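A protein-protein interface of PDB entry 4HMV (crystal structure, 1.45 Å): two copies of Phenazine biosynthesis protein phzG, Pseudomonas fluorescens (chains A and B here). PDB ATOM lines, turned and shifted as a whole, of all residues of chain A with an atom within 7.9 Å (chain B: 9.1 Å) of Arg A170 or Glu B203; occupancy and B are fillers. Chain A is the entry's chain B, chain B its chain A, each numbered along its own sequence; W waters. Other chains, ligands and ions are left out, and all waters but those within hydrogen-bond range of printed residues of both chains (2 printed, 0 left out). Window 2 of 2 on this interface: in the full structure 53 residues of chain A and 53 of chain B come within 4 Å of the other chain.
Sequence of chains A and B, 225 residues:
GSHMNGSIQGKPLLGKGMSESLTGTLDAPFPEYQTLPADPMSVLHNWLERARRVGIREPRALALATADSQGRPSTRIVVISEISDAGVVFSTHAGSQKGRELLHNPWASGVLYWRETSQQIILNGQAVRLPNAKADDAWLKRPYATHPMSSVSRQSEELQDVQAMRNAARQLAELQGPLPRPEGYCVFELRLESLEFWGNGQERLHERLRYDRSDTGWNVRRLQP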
ATOM      1  N   ALA A 145     -17.359 -18.218  -0.094  1.00  0.00           N
ATOM      2  CA  ALA A 145     -17.033 -19.552   0.424  1.00  0.00           C
ATOM      3  C   ALA A 145     -16.641 -19.527   1.903  1.00  0.00           C
ATOM      4  O   ALA A 145     -16.637 -20.568   2.562  1.00  0.00           O
ATOM      5  CB  ALA A 145     -15.907 -20.166  -0.378  1.00  0.00           C
ATOM      6  N   THR A 146     -16.278 -18.353   2.417  1.00  0.00           N
ATOM      7  CA  THR A 146     -15.902 -18.241   3.820  1.00  0.00           C
ATOM      8  C   THR A 146     -17.135 -18.007   4.694  1.00  0.00           C
ATOM      9  O   THR A 146     -17.062 -18.122   5.925  1.00  0.00           O
ATOM     10  CB  THR A 146     -14.899 -17.080   4.064  1.00  0.00           C
ATOM     11  OG1 THR A 146     -15.564 -15.817   3.922  1.00  0.00           O
ATOM     12  CG2 THR A 146     -13.731 -17.152   3.089  1.00  0.00           C
ATOM     13  N   PRO A 148     -20.136 -19.622   5.176  1.00  0.00           N
ATOM     14  CA  PRO A 148     -20.830 -20.629   5.992  1.00  0.00           C
ATOM     15  C   PRO A 148     -20.160 -20.918   7.342  1.00  0.00           C
ATOM     16  O   PRO A 148     -20.833 -20.900   8.382  1.00  0.00           O
ATOM     17  CB  PRO A 148     -20.825 -21.876   5.090  1.00  0.00           C
ATOM     18  CG  PRO A 148     -20.894 -21.305   3.712  1.00  0.00           C
ATOM     19  CD  PRO A 148     -19.960 -20.075   3.783  1.00  0.00           C
ATOM     20  N   MET A 149     -18.855 -21.163   7.345  1.00  0.00           N
ATOM     21  CA  MET A 149     -18.201 -21.533   8.597  1.00  0.00           C
ATOM     22  C   MET A 149     -18.189 -20.345   9.551  1.00  0.00           C
ATOM     23  O   MET A 149     -18.344 -20.514  10.774  1.00  0.00           O
ATOM     24  CB  MET A 149     -16.781 -22.061   8.376  1.00  0.00           C
ATOM     25  CG  MET A 149     -16.206 -22.756   9.606  1.00  0.00           C
ATOM     26  SD  MET A 149     -17.136 -24.241  10.046  1.00  0.00           S
ATOM     27  CE  MET A 149     -16.831 -25.218   8.580  1.00  0.00           C
ATOM     28  N   SER A 150     -18.006 -19.142   9.002  1.00  0.00           N
ATOM     29  CA  SER A 150     -17.959 -17.951   9.852  1.00  0.00           C
ATOM     30  C   SER A 150     -19.327 -17.650  10.445  1.00  0.00           C
ATOM     31  O   SER A 150     -19.428 -16.922  11.429  1.00  0.00           O
ATOM     32  CB  SER A 150     -17.454 -16.730   9.079  1.00  0.00           C
ATOM     33  OG  SER A 150     -16.122 -16.904   8.655  1.00  0.00           O
ATOM     34  N   VAL A 152     -21.654 -20.256  11.281  1.00  0.00           N
ATOM     35  CA  VAL A 152     -22.029 -21.271  12.255  1.00  0.00           C
ATOM     36  C   VAL A 152     -21.118 -21.231  13.480  1.00  0.00           C
ATOM     37  O   VAL A 152     -21.528 -21.592  14.567  1.00  0.00           O
ATOM     38  CB  VAL A 152     -22.045 -22.705  11.643  1.00  0.00           C
ATOM     39  CG1 VAL A 152     -23.106 -22.824  10.547  1.00  0.00           C
ATOM     40  CG2 VAL A 152     -20.692 -23.101  11.105  1.00  0.00           C
ATOM     41  N   GLN A 163     -18.050 -32.812  13.795  1.00  0.00           N
ATOM     42  CA  GLN A 163     -18.856 -33.230  12.659  1.00  0.00           C
ATOM     43  C   GLN A 163     -20.142 -32.422  12.561  1.00  0.00           C
ATOM     44  O   GLN A 163     -20.583 -32.100  11.450  1.00  0.00           O
ATOM     45  CB  GLN A 163     -19.146 -34.736  12.723  1.00  0.00           C
ATOM     46  CG  GLN A 163     -19.630 -35.303  11.380  1.00  0.00           C
ATOM     47  CD  GLN A 163     -18.567 -35.151  10.286  1.00  0.00           C
ATOM     48  OE1 GLN A 163     -17.366 -35.291  10.549  1.00  0.00           O
ATOM     49  NE2 GLN A 163     -19.000 -34.844   9.069  1.00  0.00           N
ATOM     50  N   ALA A 164     -20.729 -32.066  13.702  1.00  0.00           N
ATOM     51  CA  ALA A 164     -21.977 -31.283  13.700  1.00  0.00           C
ATOM     52  C   ALA A 164     -21.738 -29.916  13.080  1.00  0.00           C
ATOM     53  O   ALA A 164     -22.562 -29.410  12.316  1.00  0.00           O
ATOM     54  CB  ALA A 164     -22.526 -31.109  15.097  1.00  0.00           C
ATOM     55  N   MET A 165     -20.609 -29.295  13.427  1.00  0.00           N
ATOM     56  CA  MET A 165     -20.293 -28.008  12.847  1.00  0.00           C
ATOM     57  C   MET A 165     -20.006 -28.152  11.347  1.00  0.00           C
ATOM     58  O   MET A 165     -20.458 -27.341  10.525  1.00  0.00           O
ATOM     59  CB  MET A 165     -19.115 -27.389  13.577  1.00  0.00           C
ATOM     60  CG  MET A 165     -18.685 -26.073  12.914  1.00  0.00           C
ATOM     61  SD  MET A 165     -17.462 -25.127  13.832  1.00  0.00           S
ATOM     62  CE  MET A 165     -18.538 -24.489  15.109  1.00  0.00           C
ATOM     63  N   ARG A 166     -19.260 -29.188  10.989  1.00  0.00           N
ATOM     64  CA  ARG A 166     -18.950 -29.451   9.589  1.00  0.00           C
ATOM     65  C   ARG A 166     -20.242 -29.641   8.776  1.00  0.00           C
ATOM     66  O   ARG A 166     -20.412 -29.030   7.704  1.00  0.00           O
ATOM     67  CB  ARG A 166     -18.057 -30.680   9.467  1.00  0.00           C
ATOM     68  CG  ARG A 166     -17.351 -30.784   8.135  1.00  0.00           C
ATOM     69  CD  ARG A 166     -16.354 -31.936   8.072  1.00  0.00           C
ATOM     70  NE  ARG A 166     -15.243 -31.842   9.031  1.00  0.00           N
ATOM     71  CZ  ARG A 166     -14.213 -30.986   8.951  1.00  0.00           C
ATOM     72  NH1 ARG A 166     -14.120 -30.087   7.972  1.00  0.00           N
ATOM     73  NH2 ARG A 166     -13.272 -31.026   9.874  1.00  0.00           N
ATOM     74  N   ASN A 167     -21.161 -30.455   9.294  1.00  0.00           N
ATOM     75  CA  ASN A 167     -22.395 -30.736   8.575  1.00  0.00           C
ATOM     76  C   ASN A 167     -23.280 -29.494   8.445  1.00  0.00           C
ATOM     77  O   ASN A 167     -23.902 -29.252   7.393  1.00  0.00           O
ATOM     78  CB  ASN A 167     -23.165 -31.858   9.264  1.00  0.00           C
ATOM     79  CG  ASN A 167     -22.492 -33.220   9.104  1.00  0.00           C
ATOM     80  OD1 ASN A 167     -21.703 -33.434   8.183  1.00  0.00           O
ATOM     81  ND2 ASN A 167     -22.824 -34.155   9.992  1.00  0.00           N
ATOM     82  N   ALA A 168     -23.372 -28.724   9.526  1.00  0.00           N
ATOM     83  CA  ALA A 168     -24.139 -27.469   9.490  1.00  0.00           C
ATOM     84  C   ALA A 168     -23.590 -26.502   8.440  1.00  0.00           C
ATOM     85  O   ALA A 168     -24.344 -25.922   7.660  1.00  0.00           O
ATOM     86  CB  ALA A 168     -24.169 -26.819  10.851  1.00  0.00           C
ATOM     87  N   ALA A 169     -22.273 -26.319   8.405  1.00  0.00           N
ATOM     88  CA  ALA A 169     -21.687 -25.405   7.434  1.00  0.00           C
ATOM     89  C   ALA A 169     -21.924 -25.902   6.008  1.00  0.00           C
ATOM     90  O   ALA A 169     -22.225 -25.109   5.117  1.00  0.00           O
ATOM     91  CB  ALA A 169     -20.186 -25.241   7.693  1.00  0.00           C
ATOM     92  N   ARG A 170     -21.785 -27.208   5.788  1.00  0.00           N
ATOM     93  CA  ARG A 170     -22.030 -27.772   4.460  1.00  0.00           C
ATOM     94  C   ARG A 170     -23.448 -27.471   3.974  1.00  0.00           C
ATOM     95  O   ARG A 170     -23.661 -27.167   2.804  1.00  0.00           O
ATOM     96  CB  ARG A 170     -21.795 -29.281   4.458  1.00  0.00           C
ATOM     97  CG  ARG A 170     -20.347 -29.657   4.501  1.00  0.00           C
ATOM     98  CD  ARG A 170     -20.196 -31.167   4.508  1.00  0.00           C
ATOM     99  NE  ARG A 170     -18.793 -31.560   4.511  1.00  0.00           N
ATOM    100  CZ  ARG A 170     -18.367 -32.776   4.828  1.00  0.00           C
ATOM    101  NH1 ARG A 170     -19.242 -33.722   5.169  1.00  0.00           N
ATOM    102  NH2 ARG A 170     -17.071 -33.052   4.800  1.00  0.00           N
ATOM    103  N   GLN A 171     -24.420 -27.549   4.869  1.00  0.00           N
ATOM    104  CA  GLN A 171     -25.788 -27.242   4.492  1.00  0.00           C
ATOM    105  C   GLN A 171     -25.918 -25.772   4.058  1.00  0.00           C
ATOM    106  O   GLN A 171     -26.608 -25.470   3.072  1.00  0.00           O
ATOM    107  CB  GLN A 171     -26.749 -27.570   5.642  1.00  0.00           C
ATOM    108  CG  GLN A 171     -28.188 -27.531   5.230  1.00  0.00           C
ATOM    109  CD  GLN A 171     -28.474 -28.478   4.078  1.00  0.00           C
ATOM    110  OE1 GLN A 171     -28.003 -29.626   4.064  1.00  0.00           O
ATOM    111  NE2 GLN A 171     -29.238 -28.003   3.096  1.00  0.00           N
ATOM    112  N   LEU A 172     -25.244 -24.861   4.761  1.00  0.00           N
ATOM    113  CA  LEU A 172     -25.345 -23.443   4.421  1.00  0.00           C
ATOM    114  C   LEU A 172     -24.622 -23.165   3.124  1.00  0.00           C
ATOM    115  O   LEU A 172     -24.984 -22.249   2.374  1.00  0.00           O
ATOM    116  CB  LEU A 172     -24.734 -22.563   5.516  1.00  0.00           C
ATOM    117  CG  LEU A 172     -25.551 -22.335   6.785  1.00  0.00           C
ATOM    118  CD1 LEU A 172     -24.740 -21.429   7.714  1.00  0.00           C
ATOM    119  CD2 LEU A 172     -26.947 -21.744   6.473  1.00  0.00           C
ATOM    120  N   ALA A 173     -23.601 -23.965   2.854  1.00  0.00           N
ATOM    121  CA  ALA A 173     -22.755 -23.744   1.693  1.00  0.00           C
ATOM    122  C   ALA A 173     -23.464 -24.102   0.399  1.00  0.00           C
ATOM    123  O   ALA A 173     -22.995 -23.765  -0.673  1.00  0.00           O
ATOM    124  CB  ALA A 173     -21.458 -24.528   1.830  1.00  0.00           C
ATOM    125  N   GLU A 174     -24.604 -24.780   0.499  1.00  0.00           N
ATOM    126  CA  GLU A 174     -25.356 -25.139  -0.696  1.00  0.00           C
ATOM    127  C   GLU A 174     -25.843 -23.895  -1.455  1.00  0.00           C
ATOM    128  O   GLU A 174     -25.977 -23.920  -2.677  1.00  0.00           O
ATOM    129  CB  GLU A 174     -26.532 -26.043  -0.331  1.00  0.00           C
ATOM    130  CG  GLU A 174     -26.112 -27.357   0.330  1.00  0.00           C
ATOM    131  N   LEU A 175     -26.095 -22.810  -0.730  1.00  0.00           N
ATOM    132  CA  LEU A 175     -26.558 -21.567  -1.342  1.00  0.00           C
ATOM    133  C   LEU A 175     -25.650 -21.107  -2.489  1.00  0.00           C
ATOM    134  O   LEU A 175     -26.128 -20.612  -3.510  1.00  0.00           O
ATOM    135  CB  LEU A 175     -26.646 -20.452  -0.289  1.00  0.00           C
ATOM    136  CG  LEU A 175     -27.119 -19.106  -0.847  1.00  0.00           C
ATOM    137  CD1 LEU A 175     -28.478 -19.262  -1.555  1.00  0.00           C
ATOM    138  CD2 LEU A 175     -27.189 -18.061   0.254  1.00  0.00           C
ATOM    139  N   GLN A 176     -24.341 -21.254  -2.314  1.00  0.00           N
ATOM    140  CA  GLN A 176     -23.398 -20.858  -3.359  1.00  0.00           C
ATOM    141  C   GLN A 176     -23.542 -19.369  -3.667  1.00  0.00           C
ATOM    142  O   GLN A 176     -23.576 -18.963  -4.830  1.00  0.00           O
ATOM    143  CB  GLN A 176     -23.639 -21.679  -4.635  1.00  0.00           C
ATOM    144  N   ASN B 200      -4.904 -25.187   9.757  1.00  0.00           N
ATOM    145  CA  ASN B 200      -5.881 -24.675   8.800  1.00  0.00           C
ATOM    146  C   ASN B 200      -7.097 -25.586   8.650  1.00  0.00           C
ATOM    147  O   ASN B 200      -8.177 -25.101   8.347  1.00  0.00           O
ATOM    148  CB  ASN B 200      -5.234 -24.474   7.429  1.00  0.00           C
ATOM    149  CG  ASN B 200      -6.065 -23.616   6.508  1.00  0.00           C
ATOM    150  OD1 ASN B 200      -6.578 -22.567   6.896  1.00  0.00           O
ATOM    151  ND2 ASN B 200      -6.215 -24.071   5.271  1.00  0.00           N
ATOM    152  N   GLY B 201      -6.922 -26.892   8.857  1.00  0.00           N
ATOM    153  CA  GLY B 201      -8.018 -27.832   8.742  1.00  0.00           C
ATOM    154  C   GLY B 201      -8.586 -27.954   7.342  1.00  0.00           C
ATOM    155  O   GLY B 201      -7.955 -27.544   6.363  1.00  0.00           O
ATOM    156  N   GLN B 202      -9.790 -28.529   7.268  1.00  0.00           N
ATOM    157  CA  GLN B 202     -10.520 -28.740   6.013  1.00  0.00           C
ATOM    158  C   GLN B 202     -11.814 -27.913   6.005  1.00  0.00           C
ATOM    159  O   GLN B 202     -12.475 -27.761   7.043  1.00  0.00           O
ATOM    160  CB  GLN B 202     -10.880 -30.220   5.876  1.00  0.00           C
ATOM    161  CG  GLN B 202      -9.717 -31.161   6.169  1.00  0.00           C
ATOM    162  CD  GLN B 202      -8.616 -31.033   5.148  1.00  0.00           C
ATOM    163  OE1 GLN B 202      -8.884 -30.981   3.946  1.00  0.00           O
ATOM    164  NE2 GLN B 202      -7.364 -30.976   5.614  1.00  0.00           N
ATOM    165  N   GLU B 203     -12.168 -27.378   4.837  1.00  0.00           N
ATOM    166  CA  GLU B 203     -13.421 -26.645   4.651  1.00  0.00           C
ATOM    167  C   GLU B 203     -13.547 -25.434   5.568  1.00  0.00           C
ATOM    168  O   GLU B 203     -14.644 -25.023   5.927  1.00  0.00           O
ATOM    169  CB  GLU B 203     -14.616 -27.590   4.827  1.00  0.00           C
ATOM    170  CG  GLU B 203     -14.563 -28.756   3.853  1.00  0.00           C
ATOM    171  CD  GLU B 203     -15.560 -29.862   4.154  1.00  0.00           C
ATOM    172  OE1 GLU B 203     -16.021 -29.986   5.313  1.00  0.00           O
ATOM    173  OE2 GLU B 203     -15.864 -30.627   3.214  1.00  0.00           O
ATOM    174  N   ARG B 204     -12.404 -24.869   5.932  1.00  0.00           N
ATOM    175  CA  ARG B 204     -12.326 -23.675   6.772  1.00  0.00           C
ATOM    176  C   ARG B 204     -12.675 -23.940   8.233  1.00  0.00           C
ATOM    177  O   ARG B 204     -12.749 -23.003   9.059  1.00  0.00           O
ATOM    178  CB  ARG B 204     -13.152 -22.534   6.169  1.00  0.00           C
ATOM    179  CG  ARG B 204     -12.684 -22.238   4.746  1.00  0.00           C
ATOM    180  CD  ARG B 204     -13.333 -21.034   4.120  1.00  0.00           C
ATOM    181  NE  ARG B 204     -13.146 -21.053   2.667  1.00  0.00           N
ATOM    182  CZ  ARG B 204     -12.107 -20.530   2.019  1.00  0.00           C
ATOM    183  NH1 ARG B 204     -11.131 -19.913   2.672  1.00  0.00           N
ATOM    184  NH2 ARG B 204     -12.053 -20.616   0.698  1.00  0.00           N
ATOM    185  N   LEU B 205     -12.856 -25.213   8.567  1.00  0.00           N
ATOM    186  CA  LEU B 205     -13.024 -25.586   9.959  1.00  0.00           C
ATOM    187  C   LEU B 205     -11.627 -25.671  10.546  1.00  0.00           C
ATOM    188  O   LEU B 205     -11.016 -26.740  10.662  1.00  0.00           O
ATOM    189  CB  LEU B 205     -13.798 -26.894  10.108  1.00  0.00           C
ATOM    190  CG  LEU B 205     -14.565 -27.018  11.423  1.00  0.00           C
ATOM    191  CD1 LEU B 205     -15.513 -28.213  11.345  1.00  0.00           C
ATOM    192  CD2 LEU B 205     -13.639 -27.117  12.626  1.00  0.00           C
ATOM    193  N   HIS B 206     -11.117 -24.511  10.921  1.00  0.00           N
ATOM    194  CA  HIS B 206      -9.761 -24.451  11.415  1.00  0.00           C
ATOM    195  C   HIS B 206      -9.713 -25.224  12.720  1.00  0.00           C
ATOM    196  O   HIS B 206     -10.658 -25.218  13.517  1.00  0.00           O
ATOM    197  CB  HIS B 206      -9.292 -23.011  11.600  1.00  0.00           C
ATOM    198  CG  HIS B 206      -9.515 -22.159  10.404  1.00  0.00           C
ATOM    199  ND1 HIS B 206      -9.138 -22.541   9.140  1.00  0.00           N
ATOM    200  CD2 HIS B 206     -10.100 -20.943  10.274  1.00  0.00           C
ATOM    201  CE1 HIS B 206      -9.446 -21.584   8.282  1.00  0.00           C
ATOM    202  NE2 HIS B 206     -10.036 -20.606   8.943  1.00  0.00           N
ATOM    203  N   GLU B 207      -8.616 -25.931  12.900  1.00  0.00           N
ATOM    204  CA  GLU B 207      -8.454 -26.886  13.984  1.00  0.00           C
ATOM    205  C   GLU B 207      -7.686 -26.245  15.129  1.00  0.00           C
ATOM    206  O   GLU B 207      -6.548 -25.817  14.953  1.00  0.00           O
ATOM    207  CB  GLU B 207      -7.763 -28.129  13.433  1.00  0.00           C
ATOM    208  CG  GLU B 207      -8.662 -28.791  12.395  1.00  0.00           C
ATOM    209  CD  GLU B 207      -8.093 -30.009  11.723  1.00  0.00           C
ATOM    210  OE1 GLU B 207      -6.889 -30.318  11.918  1.00  0.00           O
ATOM    211  OE2 GLU B 207      -8.873 -30.667  10.981  1.00  0.00           O
ATOM    212  N   PRO B 225     -13.617 -22.303  15.366  1.00  0.00           N
ATOM    213  CA  PRO B 225     -12.707 -21.472  14.562  1.00  0.00           C
ATOM    214  C   PRO B 225     -13.114 -20.018  14.415  1.00  0.00           C
ATOM    215  O   PRO B 225     -12.202 -19.202  14.168  1.00  0.00           O
ATOM    216  CB  PRO B 225     -12.728 -22.144  13.201  1.00  0.00           C
ATOM    217  CG  PRO B 225     -13.998 -22.908  13.170  1.00  0.00           C
ATOM    218  CD  PRO B 225     -14.270 -23.343  14.556  1.00  0.00           C
ATOM    219  OXT PRO B 225     -14.302 -19.628  14.518  1.00  0.00           O
HETATM  220  O   HOH W   1     -18.220 -27.947   6.218  1.00  0.00           O
HETATM  221  O   HOH W   2     -10.894 -29.322   9.858  1.00  0.00           O
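OE2 of Glu B203 lies within salt-bridge range of NH2 of Arg A170 (3.1 Å).
The backbone carbonyl oxygen of Gln B202 is in hydrogen-bond range of the guanidinium group of Arg A166, at 3.0 Å.
The guanidinium group (NH1) of Arg A166 is in salt-bridge range of the side-chain carboxylate (OE1) of Glu B203 (3.3 Å).
O of Thr A146 sits at hydrogen-bond distance from OG of Ser A150.
Among the printed residues, pairs that only touch across the chains: Ala A145 with Arg B204 (3.5 Å), Thr A146 with Arg B204 (3.8 Å), Met A149 with Glu B203 (3.4 Å), Met A149 with Arg B204 (3.5 Å), Met A149 with Leu B205 (3.8 Å), Met A165 with Pro B225 (3.7 Å) and Arg A166 with Leu B205 (3.9 Å).
Of the printed residues of chain B, Ala A145 touches Arg B204.
Of the printed residues of chain B, Met A149 touches Glu B203, Arg B204 and Leu B205.
No residue of chain B comes within 4 Å of Ala A169.
No residue of chain B comes within 4 Å of Ala A173.
Glu B203 touches just these residues of chain A: Met A149 (3.4 Å), Arg A166 (3.2 Å) and Arg A170 (3.1 Å).
Printed residues of chain A within 4 Å of Leu B205: Met A149 and Arg A166.
Of the printed residues of chain A, Pro B225 touches Met A165 (3.7 Å).
The nearest printed residue of chain A that does not touch Arg B204 is Arg A166 (5.9 Å).
Hydrophobic or aromatic side chains of chain A within 4 Å of the printed part of chain B: Met A149 and Met A165.
Of the 9 printed residues of chain B, 5 touch a printed residue of chain A.
Printed residues of chain B that touch a printed residue of chain A: Gln B202, Glu B203, Arg B204, Leu B205 and Pro B225.
Hydrophobic or aromatic side chains of chain B within 4 Å of the printed part of chain A: Leu B205 and Pro B225.
Among the printed residues, 10 pairs touch across the chains.
Among the printed residues, Asp or Glu carboxylates within 4 Å of a Lys or Arg side-chain nitrogen of the other chain: Arg A166 with Glu B203 (3.3 Å) and Arg A170 with Glu B203 (3.1 Å).
No position is printed for both chains.
Water W2 lies within hydrogen-bond range of the side-chain carboxylate of Glu B207 (2.7 Å), the backbone carbonyl oxygen of Leu B205 (2.7 Å), the backbone NH of Gln B202 (2.9 Å) and the guanidinium group of Arg A166 (2.9 Å).
Water W1 bridges the backbone carbonyl oxygen (O) of Arg A166 (2.9 Å) and the side-chain carboxylate (OE1) of Glu B203 (3.1 Å).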
